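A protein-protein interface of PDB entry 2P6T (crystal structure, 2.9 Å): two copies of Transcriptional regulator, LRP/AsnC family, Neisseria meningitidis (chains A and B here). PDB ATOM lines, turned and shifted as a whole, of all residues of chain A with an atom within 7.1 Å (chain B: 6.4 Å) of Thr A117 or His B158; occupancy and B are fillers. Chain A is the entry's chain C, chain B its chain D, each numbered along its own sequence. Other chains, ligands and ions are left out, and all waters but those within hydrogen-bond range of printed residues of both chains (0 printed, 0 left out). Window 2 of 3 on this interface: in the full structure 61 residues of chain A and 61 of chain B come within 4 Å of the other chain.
The backbone carbonyl oxygen (O) of Val A66 lies within hydrogen-bond range of a ring nitrogen (NE2) of His B158 (2.5 Å).
O of Pro A63 sits at hydrogen-bond distance from N of Leu A68 (3.0 Å). The backbone carbonyl oxygen of Pro B155 lies close to a ring nitrogen (ND1) of His B158 (3.3 Å).
Val A66 touches Leu B156 (CB to CD2, 3.8 Å). Leu B159 touches Val A66 (CD2 to O, 3.6 Å). O of Pro B155 touches CD1 of Leu A68 (3.5 Å). His B158 touches Leu A68 (NE2 to CD2, 3.4 Å). His B158 touches Thr A117 (CD2 to CG2, 3.5 Å).
Of chain B, only His B158 comes within 4 Å of Thr A117. His B158 touches just these residues of chain A: Val A66 (2.5 Å), Leu A68 (3.4 Å) and Thr A117 (3.5 Å). Printed residues of chain B within 4 Å of Val A66: Leu B156, His B158 and Leu B159. Of the printed residues of chain A, Leu B159 touches Val A66. Of the printed residues of chain A, Pro B155 touches Leu A68 (3.5 Å). Asp A118 touches none of the printed residues of chain B. The nearest residue of chain B that does not touch Thr A117 is Leu B159 (6.3 Å). The nearest printed residue of chain B that does not touch Leu A68 is Leu B156 (5.7 Å).
Of the 15 printed residues of chain A, 3 touch a printed residue of chain B. Hydrophobic or aromatic side chains of chain A that line the printed part of chain B: Val A66 and Leu A68. Along chain A the printed residues that touch a printed residue of chain B span positions 66 to 117. Of the 7 printed residues of chain B, 4 touch a printed residue of chain A. Hydrophobic or aromatic side chains of chain B that line the printed part of chain A: Leu B156, His B158 and Leu B159. Among the printed residues, 6 pairs touch across the chains.
No position is printed for both chains.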
ATOM      1  N   PRO A  63     -12.955   3.646  19.688  1.00  0.00           N
ATOM      2  CA  PRO A  63     -12.934   4.288  21.002  1.00  0.00           C
ATOM      3  C   PRO A  63     -11.981   3.635  22.001  1.00  0.00           C
ATOM      4  O   PRO A  63     -11.119   4.305  22.569  1.00  0.00           O
ATOM      5  CB  PRO A  63     -14.382   4.155  21.465  1.00  0.00           C
ATOM      6  CG  PRO A  63     -15.152   4.205  20.219  1.00  0.00           C
ATOM      7  CD  PRO A  63     -14.337   3.475  19.206  1.00  0.00           C
ATOM      8  N   SER A  65      -9.472   1.875  21.497  1.00  0.00           N
ATOM      9  CA  SER A  65      -8.097   2.113  21.062  1.00  0.00           C
ATOM     10  C   SER A  65      -7.604   3.467  21.533  1.00  0.00           C
ATOM     11  O   SER A  65      -6.433   3.617  21.844  1.00  0.00           O
ATOM     12  CB  SER A  65      -7.985   2.069  19.544  1.00  0.00           C
ATOM     13  OG  SER A  65      -8.310   3.343  19.004  1.00  0.00           O
ATOM     14  N   VAL A  66      -8.498   4.452  21.575  1.00  0.00           N
ATOM     15  CA  VAL A  66      -8.125   5.800  21.992  1.00  0.00           C
ATOM     16  C   VAL A  66      -8.449   6.080  23.467  1.00  0.00           C
ATOM     17  O   VAL A  66      -8.508   7.240  23.882  1.00  0.00           O
ATOM     18  CB  VAL A  66      -8.770   6.858  21.077  1.00  0.00           C
ATOM     19  CG1 VAL A  66      -8.616   6.428  19.621  1.00  0.00           C
ATOM     20  CG2 VAL A  66     -10.239   7.078  21.427  1.00  0.00           C
ATOM     21  N   ASN A  67      -8.639   5.005  24.239  1.00  0.00           N
ATOM     22  CA  ASN A  67      -8.843   5.041  25.698  1.00  0.00           C
ATOM     23  C   ASN A  67     -10.214   5.545  26.171  1.00  0.00           C
ATOM     24  O   ASN A  67     -10.417   5.788  27.364  1.00  0.00           O
ATOM     25  CB  ASN A  67      -7.717   5.814  26.390  1.00  0.00           C
ATOM     26  CG  ASN A  67      -7.653   5.538  27.879  1.00  0.00           C
ATOM     27  OD1 ASN A  67      -8.069   4.474  28.349  1.00  0.00           O
ATOM     28  ND2 ASN A  67      -7.138   6.505  28.633  1.00  0.00           N
ATOM     29  N   LEU A  68     -11.158   5.661  25.244  1.00  0.00           N
ATOM     30  CA  LEU A  68     -12.532   6.015  25.581  1.00  0.00           C
ATOM     31  C   LEU A  68     -13.365   4.737  25.752  1.00  0.00           C
ATOM     32  O   LEU A  68     -13.924   4.200  24.793  1.00  0.00           O
ATOM     33  CB  LEU A  68     -13.112   6.933  24.501  1.00  0.00           C
ATOM     34  CG  LEU A  68     -12.261   8.186  24.241  1.00  0.00           C
ATOM     35  CD1 LEU A  68     -12.818   9.038  23.110  1.00  0.00           C
ATOM     36  CD2 LEU A  68     -12.131   9.008  25.509  1.00  0.00           C
ATOM     37  N   GLY A  69     -13.421   4.240  26.983  1.00  0.00           N
ATOM     38  CA  GLY A  69     -14.152   3.014  27.280  1.00  0.00           C
ATOM     39  C   GLY A  69     -15.627   3.247  27.554  1.00  0.00           C
ATOM     40  O   GLY A  69     -16.443   2.351  27.346  1.00  0.00           O
ATOM     41  N   LEU A  70     -15.975   4.444  28.015  1.00  0.00           N
ATOM     42  CA  LEU A  70     -17.332   4.723  28.452  1.00  0.00           C
ATOM     43  C   LEU A  70     -18.123   5.495  27.389  1.00  0.00           C
ATOM     44  O   LEU A  70     -17.967   6.712  27.223  1.00  0.00           O
ATOM     45  CB  LEU A  70     -17.309   5.480  29.789  1.00  0.00           C
ATOM     46  CG  LEU A  70     -18.514   5.314  30.730  1.00  0.00           C
ATOM     47  CD1 LEU A  70     -18.637   3.879  31.246  1.00  0.00           C
ATOM     48  CD2 LEU A  70     -18.421   6.281  31.910  1.00  0.00           C
ATOM     49  N   PHE A 115     -18.712  10.256  24.690  1.00  0.00           N
ATOM     50  CA  PHE A 115     -17.684   9.285  25.050  1.00  0.00           C
ATOM     51  C   PHE A 115     -16.750   9.842  26.103  1.00  0.00           C
ATOM     52  O   PHE A 115     -16.462  11.046  26.130  1.00  0.00           O
ATOM     53  CB  PHE A 115     -16.864   8.897  23.824  1.00  0.00           C
ATOM     54  CG  PHE A 115     -17.543   7.900  22.931  1.00  0.00           C
ATOM     55  CD1 PHE A 115     -17.030   6.616  22.784  1.00  0.00           C
ATOM     56  CD2 PHE A 115     -18.696   8.248  22.231  1.00  0.00           C
ATOM     57  CE1 PHE A 115     -17.647   5.706  21.955  1.00  0.00           C
ATOM     58  CE2 PHE A 115     -19.322   7.342  21.403  1.00  0.00           C
ATOM     59  CZ  PHE A 115     -18.795   6.069  21.262  1.00  0.00           C
ATOM     60  N   PHE A 116     -16.267   8.948  26.959  1.00  0.00           N
ATOM     61  CA  PHE A 116     -15.375   9.319  28.044  1.00  0.00           C
ATOM     62  C   PHE A 116     -14.353   8.230  28.314  1.00  0.00           C
ATOM     63  O   PHE A 116     -14.478   7.096  27.837  1.00  0.00           O
ATOM     64  CB  PHE A 116     -16.184   9.586  29.312  1.00  0.00           C
ATOM     65  CG  PHE A 116     -17.263  10.605  29.125  1.00  0.00           C
ATOM     66  CD1 PHE A 116     -16.974  11.960  29.199  1.00  0.00           C
ATOM     67  CD2 PHE A 116     -18.560  10.212  28.840  1.00  0.00           C
ATOM     68  CE1 PHE A 116     -17.966  12.905  29.014  1.00  0.00           C
ATOM     69  CE2 PHE A 116     -19.555  11.148  28.649  1.00  0.00           C
ATOM     70  CZ  PHE A 116     -19.261  12.497  28.742  1.00  0.00           C
ATOM     71  N   THR A 117     -13.343   8.593  29.093  1.00  0.00           N
ATOM     72  CA  THR A 117     -12.299   7.664  29.497  1.00  0.00           C
ATOM     73  C   THR A 117     -12.819   6.648  30.515  1.00  0.00           C
ATOM     74  O   THR A 117     -12.762   5.437  30.291  1.00  0.00           O
ATOM     75  CB  THR A 117     -11.120   8.435  30.093  1.00  0.00           C
ATOM     76  OG1 THR A 117     -11.619   9.568  30.813  1.00  0.00           O
ATOM     77  CG2 THR A 117     -10.188   8.918  28.987  1.00  0.00           C
ATOM     78  N   ASP A 118     -13.340   7.167  31.622  1.00  0.00           N
ATOM     79  CA  ASP A 118     -13.836   6.351  32.730  1.00  0.00           C
ATOM     80  C   ASP A 118     -14.999   7.053  33.442  1.00  0.00           C
ATOM     81  O   ASP A 118     -15.292   8.230  33.194  1.00  0.00           O
ATOM     82  CB  ASP A 118     -12.712   6.127  33.740  1.00  0.00           C
ATOM     83  CG  ASP A 118     -12.155   7.439  34.282  1.00  0.00           C
ATOM     84  OD1 ASP A 118     -12.953   8.379  34.504  1.00  0.00           O
ATOM     85  OD2 ASP A 118     -10.921   7.536  34.468  1.00  0.00           O
ATOM     86  N   MET A 119     -15.626   6.338  34.368  1.00  0.00           N
ATOM     87  CA  MET A 119     -16.751   6.886  35.127  1.00  0.00           C
ATOM     88  C   MET A 119     -16.435   8.266  35.776  1.00  0.00           C
ATOM     89  O   MET A 119     -17.294   9.159  35.821  1.00  0.00           O
ATOM     90  CB  MET A 119     -17.225   5.866  36.173  1.00  0.00           C
ATOM     91  CG  MET A 119     -18.601   6.150  36.734  1.00  0.00           C
ATOM     92  SD  MET A 119     -20.023   6.441  35.403  1.00  0.00           S
ATOM     93  CE  MET A 119     -21.348   7.152  36.639  1.00  0.00           C
ATOM     94  N   ASN A 120     -15.209   8.445  36.253  1.00  0.00           N
ATOM     95  CA  ASN A 120     -14.832   9.709  36.871  1.00  0.00           C
ATOM     96  C   ASN A 120     -14.846  10.869  35.880  1.00  0.00           C
ATOM     97  O   ASN A 120     -15.414  11.927  36.162  1.00  0.00           O
ATOM     98  CB  ASN A 120     -13.458   9.609  37.529  1.00  0.00           C
ATOM     99  CG  ASN A 120     -13.545   9.178  38.972  1.00  0.00           C
ATOM    100  OD1 ASN A 120     -12.921   8.197  39.369  1.00  0.00           O
ATOM    101  ND2 ASN A 120     -14.335   9.901  39.768  1.00  0.00           N
ATOM    102  N   ALA A 121     -14.222  10.672  34.722  1.00  0.00           N
ATOM    103  CA  ALA A 121     -14.317  11.653  33.652  1.00  0.00           C
ATOM    104  C   ALA A 121     -15.780  12.045  33.464  1.00  0.00           C
ATOM    105  O   ALA A 121     -16.128  13.218  33.508  1.00  0.00           O
ATOM    106  CB  ALA A 121     -13.748  11.102  32.360  1.00  0.00           C
ATOM    107  N   PHE A 122     -16.641  11.052  33.290  1.00  0.00           N
ATOM    108  CA  PHE A 122     -18.063  11.303  33.116  1.00  0.00           C
ATOM    109  C   PHE A 122     -18.598  12.227  34.212  1.00  0.00           C
ATOM    110  O   PHE A 122     -19.210  13.269  33.935  1.00  0.00           O
ATOM    111  CB  PHE A 122     -18.855   9.984  33.122  1.00  0.00           C
ATOM    112  CG  PHE A 122     -20.332  10.179  32.940  1.00  0.00           C
ATOM    113  CD1 PHE A 122     -20.868  10.362  31.673  1.00  0.00           C
ATOM    114  CD2 PHE A 122     -21.178  10.232  34.031  1.00  0.00           C
ATOM    115  CE1 PHE A 122     -22.234  10.572  31.492  1.00  0.00           C
ATOM    116  CE2 PHE A 122     -22.541  10.447  33.864  1.00  0.00           C
ATOM    117  CZ  PHE A 122     -23.070  10.613  32.588  1.00  0.00           C
ATOM    118  N   ILE B  13      -1.689  12.723  17.732  1.00  0.00           N
ATOM    119  CA  ILE B  13      -3.055  13.130  18.005  1.00  0.00           C
ATOM    120  C   ILE B  13      -3.600  13.857  16.779  1.00  0.00           C
ATOM    121  O   ILE B  13      -4.616  13.460  16.198  1.00  0.00           O
ATOM    122  CB  ILE B  13      -3.109  14.081  19.230  1.00  0.00           C
ATOM    123  CG1 ILE B  13      -2.767  13.328  20.524  1.00  0.00           C
ATOM    124  CG2 ILE B  13      -4.473  14.748  19.341  1.00  0.00           C
ATOM    125  CD1 ILE B  13      -2.730  14.218  21.763  1.00  0.00           C
ATOM    126  N   PRO B 155     -13.359  12.905  20.629  1.00  0.00           N
ATOM    127  CA  PRO B 155     -12.424  13.790  21.341  1.00  0.00           C
ATOM    128  C   PRO B 155     -11.123  13.085  21.727  1.00  0.00           C
ATOM    129  O   PRO B 155     -11.170  11.984  22.267  1.00  0.00           O
ATOM    130  CB  PRO B 155     -13.202  14.160  22.606  1.00  0.00           C
ATOM    131  CG  PRO B 155     -14.127  13.029  22.805  1.00  0.00           C
ATOM    132  CD  PRO B 155     -14.561  12.644  21.440  1.00  0.00           C
ATOM    133  N   LEU B 156      -9.983  13.726  21.470  1.00  0.00           N
ATOM    134  CA  LEU B 156      -8.670  13.100  21.695  1.00  0.00           C
ATOM    135  C   LEU B 156      -7.746  13.849  22.667  1.00  0.00           C
ATOM    136  O   LEU B 156      -6.680  13.340  23.031  1.00  0.00           O
ATOM    137  CB  LEU B 156      -7.955  12.916  20.354  1.00  0.00           C
ATOM    138  CG  LEU B 156      -8.567  11.892  19.396  1.00  0.00           C
ATOM    139  CD1 LEU B 156      -8.034  12.109  17.977  1.00  0.00           C
ATOM    140  CD2 LEU B 156      -8.290  10.470  19.881  1.00  0.00           C
ATOM    141  N   ASN B 157      -8.152  15.039  23.107  1.00  0.00           N
ATOM    142  CA  ASN B 157      -7.297  15.854  23.974  1.00  0.00           C
ATOM    143  C   ASN B 157      -6.924  15.142  25.273  1.00  0.00           C
ATOM    144  O   ASN B 157      -5.934  15.488  25.911  1.00  0.00           O
ATOM    145  CB  ASN B 157      -7.955  17.207  24.268  1.00  0.00           C
ATOM    146  CG  ASN B 157      -8.100  18.069  23.023  1.00  0.00           C
ATOM    147  OD1 ASN B 157      -9.058  18.831  22.897  1.00  0.00           O
ATOM    148  ND2 ASN B 157      -7.157  17.940  22.092  1.00  0.00           N
ATOM    149  N   HIS B 158      -7.703  14.138  25.657  1.00  0.00           N
ATOM    150  CA  HIS B 158      -7.361  13.320  26.815  1.00  0.00           C
ATOM    151  C   HIS B 158      -6.051  12.539  26.643  1.00  0.00           C
ATOM    152  O   HIS B 158      -5.541  11.972  27.613  1.00  0.00           O
ATOM    153  CB  HIS B 158      -8.504  12.356  27.144  1.00  0.00           C
ATOM    154  CG  HIS B 158      -8.714  11.294  26.112  1.00  0.00           C
ATOM    155  ND1 HIS B 158      -9.257  11.555  24.873  1.00  0.00           N
ATOM    156  CD2 HIS B 158      -8.454   9.966  26.138  1.00  0.00           C
ATOM    157  CE1 HIS B 158      -9.320  10.433  24.180  1.00  0.00           C
ATOM    158  NE2 HIS B 158      -8.837   9.455  24.923  1.00  0.00           N
ATOM    159  N   LEU B 159      -5.511  12.507  25.425  1.00  0.00           N
ATOM    160  CA  LEU B 159      -4.242  11.829  25.166  1.00  0.00           C
ATOM    161  C   LEU B 159      -3.026  12.759  25.244  1.00  0.00           C
ATOM    162  O   LEU B 159      -1.892  12.295  25.118  1.00  0.00           O
ATOM    163  CB  LEU B 159      -4.282  11.139  23.800  1.00  0.00           C
ATOM    164  CG  LEU B 159      -5.413  10.130  23.569  1.00  0.00           C
ATOM    165  CD1 LEU B 159      -5.182   9.367  22.271  1.00  0.00           C
ATOM    166  CD2 LEU B 159      -5.552   9.161  24.736  1.00  0.00           C
ATOM    167  N   LEU B 160      -3.250  14.059  25.452  1.00  0.00           N
ATOM    168  CA  LEU B 160      -2.144  15.020  25.592  1.00  0.00           C
ATOM    169  C   LEU B 160      -1.651  15.061  27.044  1.00  0.00           C
ATOM    170  O   LEU B 160      -1.984  15.948  27.837  1.00  0.00           O
ATOM    171  CB  LEU B 160      -2.540  16.423  25.065  1.00  0.00           C
ATOM    172  CG  LEU B 160      -3.564  17.336  25.777  1.00  0.00           C
ATOM    173  CD1 LEU B 160      -2.882  18.452  26.572  1.00  0.00           C
ATOM    174  CD2 LEU B 160      -4.541  17.956  24.771  1.00  0.00           C
